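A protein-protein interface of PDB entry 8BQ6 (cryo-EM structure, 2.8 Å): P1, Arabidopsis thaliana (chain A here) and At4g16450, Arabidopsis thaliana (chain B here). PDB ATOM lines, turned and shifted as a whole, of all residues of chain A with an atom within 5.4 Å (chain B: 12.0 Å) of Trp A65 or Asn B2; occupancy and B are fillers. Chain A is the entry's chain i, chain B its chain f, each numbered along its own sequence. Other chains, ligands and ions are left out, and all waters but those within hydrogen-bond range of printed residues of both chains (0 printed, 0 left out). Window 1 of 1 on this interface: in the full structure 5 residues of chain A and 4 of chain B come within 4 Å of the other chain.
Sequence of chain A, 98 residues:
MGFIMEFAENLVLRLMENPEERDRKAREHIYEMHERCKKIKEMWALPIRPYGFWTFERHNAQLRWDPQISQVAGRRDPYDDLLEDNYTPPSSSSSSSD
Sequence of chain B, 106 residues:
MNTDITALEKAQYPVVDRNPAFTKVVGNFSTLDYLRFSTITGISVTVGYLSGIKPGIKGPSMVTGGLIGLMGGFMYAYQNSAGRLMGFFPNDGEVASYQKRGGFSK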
ATOM      1  N   ALA A  61     -13.666 -15.545   6.804  1.00  0.00           N
ATOM      2  CA  ALA A  61     -13.196 -16.134   8.053  1.00  0.00           C
ATOM      3  C   ALA A  61     -14.145 -15.829   9.209  1.00  0.00           C
ATOM      4  O   ALA A  61     -14.417 -16.703  10.040  1.00  0.00           O
ATOM      5  CB  ALA A  61     -11.784 -15.640   8.364  1.00  0.00           C
ATOM      6  N   GLN A  62     -14.630 -14.589   9.290  1.00  0.00           N
ATOM      7  CA  GLN A  62     -15.527 -14.180  10.404  1.00  0.00           C
ATOM      8  C   GLN A  62     -16.807 -15.027  10.407  1.00  0.00           C
ATOM      9  O   GLN A  62     -17.241 -15.421  11.490  1.00  0.00           O
ATOM     10  CB  GLN A  62     -15.838 -12.689  10.276  1.00  0.00           C
ATOM     11  CG  GLN A  62     -16.929 -12.203  11.220  1.00  0.00           C
ATOM     12  CD  GLN A  62     -16.944 -10.707  11.405  1.00  0.00           C
ATOM     13  OE1 GLN A  62     -16.625  -9.946  10.497  1.00  0.00           O
ATOM     14  NE2 GLN A  62     -17.330 -10.272  12.592  1.00  0.00           N
ATOM     15  N   LEU A  63     -17.362 -15.330   9.231  1.00  0.00           N
ATOM     16  CA  LEU A  63     -18.623 -16.061   9.156  1.00  0.00           C
ATOM     17  C   LEU A  63     -18.513 -17.482   9.693  1.00  0.00           C
ATOM     18  O   LEU A  63     -19.537 -18.087  10.023  1.00  0.00           O
ATOM     19  CB  LEU A  63     -19.115 -16.093   7.714  1.00  0.00           C
ATOM     20  CG  LEU A  63     -19.835 -14.821   7.277  1.00  0.00           C
ATOM     21  CD1 LEU A  63     -20.007 -14.790   5.772  1.00  0.00           C
ATOM     22  CD2 LEU A  63     -21.145 -14.697   7.993  1.00  0.00           C
ATOM     23  N   ARG A  64     -17.305 -18.032   9.781  1.00  0.00           N
ATOM     24  CA  ARG A  64     -17.131 -19.372  10.315  1.00  0.00           C
ATOM     25  C   ARG A  64     -16.555 -19.385  11.721  1.00  0.00           C
ATOM     26  O   ARG A  64     -16.750 -20.366  12.444  1.00  0.00           O
ATOM     27  CB  ARG A  64     -16.234 -20.198   9.388  1.00  0.00           C
ATOM     28  CG  ARG A  64     -16.416 -19.848   7.926  1.00  0.00           C
ATOM     29  CD  ARG A  64     -16.134 -21.041   7.033  1.00  0.00           C
ATOM     30  NE  ARG A  64     -14.733 -21.443   7.050  1.00  0.00           N
ATOM     31  CZ  ARG A  64     -13.761 -20.800   6.418  1.00  0.00           C
ATOM     32  NH1 ARG A  64     -14.000 -19.712   5.705  1.00  0.00           N
ATOM     33  NH2 ARG A  64     -12.517 -21.264   6.500  1.00  0.00           N
ATOM     34  N   TRP A  65     -15.872 -18.316  12.126  1.00  0.00           N
ATOM     35  CA  TRP A  65     -15.287 -18.274  13.458  1.00  0.00           C
ATOM     36  C   TRP A  65     -16.264 -17.691  14.471  1.00  0.00           C
ATOM     37  O   TRP A  65     -16.400 -18.213  15.582  1.00  0.00           O
ATOM     38  CB  TRP A  65     -13.987 -17.473  13.429  1.00  0.00           C
ATOM     39  CG  TRP A  65     -13.457 -17.147  14.781  1.00  0.00           C
ATOM     40  CD1 TRP A  65     -13.501 -15.939  15.404  1.00  0.00           C
ATOM     41  CD2 TRP A  65     -12.797 -18.040  15.683  1.00  0.00           C
ATOM     42  NE1 TRP A  65     -12.911 -16.021  16.639  1.00  0.00           N
ATOM     43  CE2 TRP A  65     -12.470 -17.303  16.834  1.00  0.00           C
ATOM     44  CE3 TRP A  65     -12.459 -19.395  15.631  1.00  0.00           C
ATOM     45  CZ2 TRP A  65     -11.821 -17.871  17.922  1.00  0.00           C
ATOM     46  CZ3 TRP A  65     -11.813 -19.956  16.713  1.00  0.00           C
ATOM     47  CH2 TRP A  65     -11.500 -19.197  17.841  1.00  0.00           C
ATOM     48  N   ASP A  66     -16.963 -16.619  14.101  1.00  0.00           N
ATOM     49  CA  ASP A  66     -17.927 -16.008  15.014  1.00  0.00           C
ATOM     50  C   ASP A  66     -18.991 -16.969  15.536  1.00  0.00           C
ATOM     51  O   ASP A  66     -19.329 -16.871  16.726  1.00  0.00           O
ATOM     52  CB  ASP A  66     -18.574 -14.784  14.351  1.00  0.00           C
ATOM     53  CG  ASP A  66     -17.840 -13.496  14.677  1.00  0.00           C
ATOM     54  OD1 ASP A  66     -16.780 -13.569  15.333  1.00  0.00           O
ATOM     55  OD2 ASP A  66     -18.322 -12.412  14.291  1.00  0.00           O
ATOM     56  N   PRO A  67     -19.567 -17.881  14.741  1.00  0.00           N
ATOM     57  CA  PRO A  67     -20.499 -18.859  15.334  1.00  0.00           C
ATOM     58  C   PRO A  67     -19.875 -19.722  16.416  1.00  0.00           C
ATOM     59  O   PRO A  67     -20.584 -20.152  17.334  1.00  0.00           O
ATOM     60  CB  PRO A  67     -20.951 -19.706  14.137  1.00  0.00           C
ATOM     61  CG  PRO A  67     -20.582 -18.960  12.938  1.00  0.00           C
ATOM     62  CD  PRO A  67     -19.549 -17.948  13.269  1.00  0.00           C
ATOM     63  N   GLN A  68     -18.573 -19.999  16.334  1.00  0.00           N
ATOM     64  CA  GLN A  68     -17.914 -20.816  17.344  1.00  0.00           C
ATOM     65  C   GLN A  68     -17.781 -20.098  18.683  1.00  0.00           C
ATOM     66  O   GLN A  68     -17.665 -20.763  19.716  1.00  0.00           O
ATOM     67  CB  GLN A  68     -16.537 -21.250  16.845  1.00  0.00           C
ATOM     68  CG  GLN A  68     -16.572 -22.205  15.671  1.00  0.00           C
ATOM     69  CD  GLN A  68     -15.196 -22.462  15.105  1.00  0.00           C
ATOM     70  OE1 GLN A  68     -14.318 -22.977  15.795  1.00  0.00           O
ATOM     71  NE2 GLN A  68     -14.993 -22.094  13.847  1.00  0.00           N
ATOM     72  N   ILE A  69     -17.787 -18.767  18.693  1.00  0.00           N
ATOM     73  CA  ILE A  69     -17.729 -17.998  19.930  1.00  0.00           C
ATOM     74  C   ILE A  69     -19.076 -17.353  20.247  1.00  0.00           C
ATOM     75  O   ILE A  69     -19.149 -16.466  21.092  1.00  0.00           O
ATOM     76  CB  ILE A  69     -16.622 -16.933  19.890  1.00  0.00           C
ATOM     77  CG1 ILE A  69     -16.634 -16.203  18.543  1.00  0.00           C
ATOM     78  CG2 ILE A  69     -15.266 -17.548  20.213  1.00  0.00           C
ATOM     79  CD1 ILE A  69     -15.874 -14.909  18.539  1.00  0.00           C
ATOM     80  N   VAL A  72     -20.094 -17.050  23.981  1.00  0.00           N
ATOM     81  CA  VAL A  72     -19.075 -16.581  24.914  1.00  0.00           C
ATOM     82  C   VAL A  72     -19.584 -15.351  25.654  1.00  0.00           C
ATOM     83  O   VAL A  72     -20.147 -14.434  25.044  1.00  0.00           O
ATOM     84  CB  VAL A  72     -17.767 -16.281  24.166  1.00  0.00           C
ATOM     85  CG1 VAL A  72     -16.851 -15.426  25.008  1.00  0.00           C
ATOM     86  CG2 VAL A  72     -17.076 -17.576  23.774  1.00  0.00           C
ATOM     87  N   FME B   1     -11.116 -21.232  26.277  1.00  0.00           N
ATOM     88  CN  FME B   1     -10.277 -22.045  26.904  1.00  0.00           C
ATOM     89  O1  FME B   1     -10.593 -22.841  27.788  1.00  0.00           O
ATOM     90  CA  FME B   1     -10.807 -20.547  25.034  1.00  0.00           C
ATOM     91  CB  FME B   1      -9.382 -19.976  25.007  1.00  0.00           C
ATOM     92  CG  FME B   1      -9.373 -18.460  25.078  1.00  0.00           C
ATOM     93  SD  FME B   1      -8.395 -17.677  23.776  1.00  0.00           S
ATOM     94  CE  FME B   1      -9.560 -17.690  22.416  1.00  0.00           C
ATOM     95  C   FME B   1     -11.094 -21.418  23.801  1.00  0.00           C
ATOM     96  O   FME B   1     -10.289 -22.399  23.669  1.00  0.00           O
ATOM     97  N   ASN B   2     -12.068 -20.953  22.985  1.00  0.00           N
ATOM     98  CA  ASN B   2     -12.452 -21.725  21.771  1.00  0.00           C
ATOM     99  C   ASN B   2     -11.281 -21.774  20.791  1.00  0.00           C
ATOM    100  O   ASN B   2     -10.628 -20.733  20.595  1.00  0.00           O
ATOM    101  CB  ASN B   2     -13.701 -21.167  21.088  1.00  0.00           C
ATOM    102  CG  ASN B   2     -14.951 -21.358  21.917  1.00  0.00           C
ATOM    103  OD1 ASN B   2     -15.611 -20.391  22.285  1.00  0.00           O
ATOM    104  ND2 ASN B   2     -15.282 -22.603  22.221  1.00  0.00           N
ATOM    105  N   THR B   3     -11.039 -22.943  20.203  1.00  0.00           N
ATOM    106  CA  THR B   3      -9.875 -23.116  19.298  1.00  0.00           C
ATOM    107  C   THR B   3     -10.310 -23.785  17.996  1.00  0.00           C
ATOM    108  O   THR B   3     -11.426 -24.347  17.957  1.00  0.00           O
ATOM    109  CB  THR B   3      -8.788 -23.957  19.973  1.00  0.00           C
ATOM    110  OG1 THR B   3      -9.335 -25.239  20.283  1.00  0.00           O
ATOM    111  CG2 THR B   3      -8.226 -23.333  21.232  1.00  0.00           C
ATOM    112  N   ASP B   4      -9.447 -23.758  16.983  1.00  0.00           N
ATOM    113  CA  ASP B   4      -9.748 -24.397  15.709  1.00  0.00           C
ATOM    114  C   ASP B   4      -8.436 -24.581  14.962  1.00  0.00           C
ATOM    115  O   ASP B   4      -7.834 -23.598  14.522  1.00  0.00           O
ATOM    116  CB  ASP B   4     -10.738 -23.565  14.911  1.00  0.00           C
ATOM    117  CG  ASP B   4     -11.541 -24.399  13.954  1.00  0.00           C
ATOM    118  OD1 ASP B   4     -11.085 -24.573  12.810  1.00  0.00           O
ATOM    119  OD2 ASP B   4     -12.615 -24.899  14.343  1.00  0.00           O
ATOM    120  N   ILE B   5      -7.999 -25.836  14.826  1.00  0.00           N
ATOM    121  CA  ILE B   5      -6.735 -26.137  14.166  1.00  0.00           C
ATOM    122  C   ILE B   5      -6.814 -26.016  12.651  1.00  0.00           C
ATOM    123  O   ILE B   5      -5.770 -25.983  11.993  1.00  0.00           O
ATOM    124  CB  ILE B   5      -6.262 -27.551  14.571  1.00  0.00           C
ATOM    125  CG1 ILE B   5      -4.748 -27.708  14.392  1.00  0.00           C
ATOM    126  CG2 ILE B   5      -7.007 -28.616  13.787  1.00  0.00           C
ATOM    127  CD1 ILE B   5      -3.926 -26.806  15.268  1.00  0.00           C
ATOM    128  N   THR B   6      -8.021 -25.919  12.089  1.00  0.00           N
ATOM    129  CA  THR B   6      -8.219 -26.004  10.645  1.00  0.00           C
ATOM    130  C   THR B   6      -7.343 -25.014   9.898  1.00  0.00           C
ATOM    131  O   THR B   6      -7.360 -23.811  10.177  1.00  0.00           O
ATOM    132  CB  THR B   6      -9.691 -25.762  10.302  1.00  0.00           C
ATOM    133  OG1 THR B   6     -10.459 -26.921  10.641  1.00  0.00           O
ATOM    134  CG2 THR B   6      -9.862 -25.458   8.820  1.00  0.00           C
ATOM    135  N   ALA B   7      -6.588 -25.526   8.939  1.00  0.00           N
ATOM    136  CA  ALA B   7      -5.671 -24.702   8.176  1.00  0.00           C
ATOM    137  C   ALA B   7      -6.352 -24.164   6.926  1.00  0.00           C
ATOM    138  O   ALA B   7      -7.363 -24.690   6.455  1.00  0.00           O
ATOM    139  CB  ALA B   7      -4.423 -25.496   7.798  1.00  0.00           C
ATOM    140  N   LEU B   8      -5.782 -23.078   6.405  1.00  0.00           N
ATOM    141  CA  LEU B   8      -6.282 -22.471   5.178  1.00  0.00           C
ATOM    142  C   LEU B   8      -6.093 -23.400   3.988  1.00  0.00           C
ATOM    143  O   LEU B   8      -6.970 -23.514   3.124  1.00  0.00           O
ATOM    144  CB  LEU B   8      -5.556 -21.154   4.942  1.00  0.00           C
ATOM    145  CG  LEU B   8      -5.923 -20.362   3.696  1.00  0.00           C
ATOM    146  CD1 LEU B   8      -7.420 -20.112   3.648  1.00  0.00           C
ATOM    147  CD2 LEU B   8      -5.130 -19.074   3.663  1.00  0.00           C
ATOM    148  N   ARG B  18      -5.177 -35.326  13.410  1.00  0.00           N
ATOM    149  CA  ARG B  18      -5.474 -33.925  13.115  1.00  0.00           C
ATOM    150  C   ARG B  18      -4.719 -32.972  14.035  1.00  0.00           C
ATOM    151  O   ARG B  18      -4.098 -32.010  13.569  1.00  0.00           O
ATOM    152  CB  ARG B  18      -6.976 -33.669  13.232  1.00  0.00           C
ATOM    153  CG  ARG B  18      -7.397 -32.272  12.827  1.00  0.00           C
ATOM    154  CD  ARG B  18      -8.906 -32.098  12.868  1.00  0.00           C
ATOM    155  NE  ARG B  18      -9.298 -30.743  12.499  1.00  0.00           N
ATOM    156  CZ  ARG B  18      -9.436 -30.309  11.253  1.00  0.00           C
ATOM    157  NH1 ARG B  18      -9.233 -31.106  10.217  1.00  0.00           N
ATOM    158  NH2 ARG B  18      -9.784 -29.043  11.042  1.00  0.00           N
ATOM    159  N   ASN B  19      -4.789 -33.205  15.343  1.00  0.00           N
ATOM    160  CA  ASN B  19      -4.189 -32.327  16.348  1.00  0.00           C
ATOM    161  C   ASN B  19      -3.365 -33.181  17.301  1.00  0.00           C
ATOM    162  O   ASN B  19      -3.770 -33.441  18.439  1.00  0.00           O
ATOM    163  CB  ASN B  19      -5.273 -31.550  17.100  1.00  0.00           C
ATOM    164  CG  ASN B  19      -4.742 -30.308  17.784  1.00  0.00           C
ATOM    165  OD1 ASN B  19      -3.593 -30.263  18.220  1.00  0.00           O
ATOM    166  ND2 ASN B  19      -5.587 -29.291  17.891  1.00  0.00           N
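OD1 of Asn B2 lies close to O of Gln A68, at 3.3 Å.
The side-chain carboxylate (OD2) of Asp B4 lies close to the side-chain amide oxygen (OE1) of Gln A68 (3.0 Å).
OG1 of Thr B6 lies close to OD1 of Asp B4, 3.3 Å away.
The backbone carbonyl oxygen of Arg A64 lies within hydrogen-bond range of the side-chain amide nitrogen of Gln A68 (2.8 Å).
Asn B2 touches Trp A65.
OE1 of Gln A68 touches O of Thr B3, at 3.9 Å.
Ile A69 touches Asn B2 (CG2 to OD1, 3.5 Å).
CG2 of Val A72 touches OD1 of Asn B2 (3.5 Å).
Of the printed residues of chain B, Trp A65 touches Asn B2.
Of chain A, only Trp A65, Gln A68, Ile A69 and Val A72 come within 4 Å of Asn B2.
No residue of chain B comes within 4 Å of Ala A61.
No residue of chain B comes within 4 Å of Arg A64.
No residue of chain B comes within 4 Å of Asp A66.
No residue of chain B comes within 4 Å of Pro A67.
Gln A68 touches three residues of chain B.
Of chain B, only Asn B2 comes within 4 Å of Ile A69.
Of the printed residues of chain A, Thr B3 touches Gln A68 (3.9 Å).
Of the printed residues of chain B, Val A72 touches Asn B2.
Thr B6 touches none of the printed residues of chain A.
Asn B19 touches none of the printed residues of chain A.
The nearest residue of chain B that does not touch Trp A65 is Asp B4 (4.2 Å).
The nearest printed residue of chain A that does not touch Asn B2 is Pro A67 (7.0 Å).
Of the 10 printed residues of chain A, 4 touch a printed residue of chain B.
Hydrophobic or aromatic side chains of chain A that line the printed part of chain B: Trp A65, Ile A69 and Val A72.
Of the 10 printed residues of chain B, 3 touch a printed residue of chain A.
Printed residues of chain B that touch a printed residue of chain A: Asn B2, Thr B3 and Asp B4.
Among the printed residues, 6 pairs touch across the chains.
Among the printed residues, no Asp or Glu carboxylate lies within 4 Å of a Lys or Arg side-chain nitrogen of the other chain.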
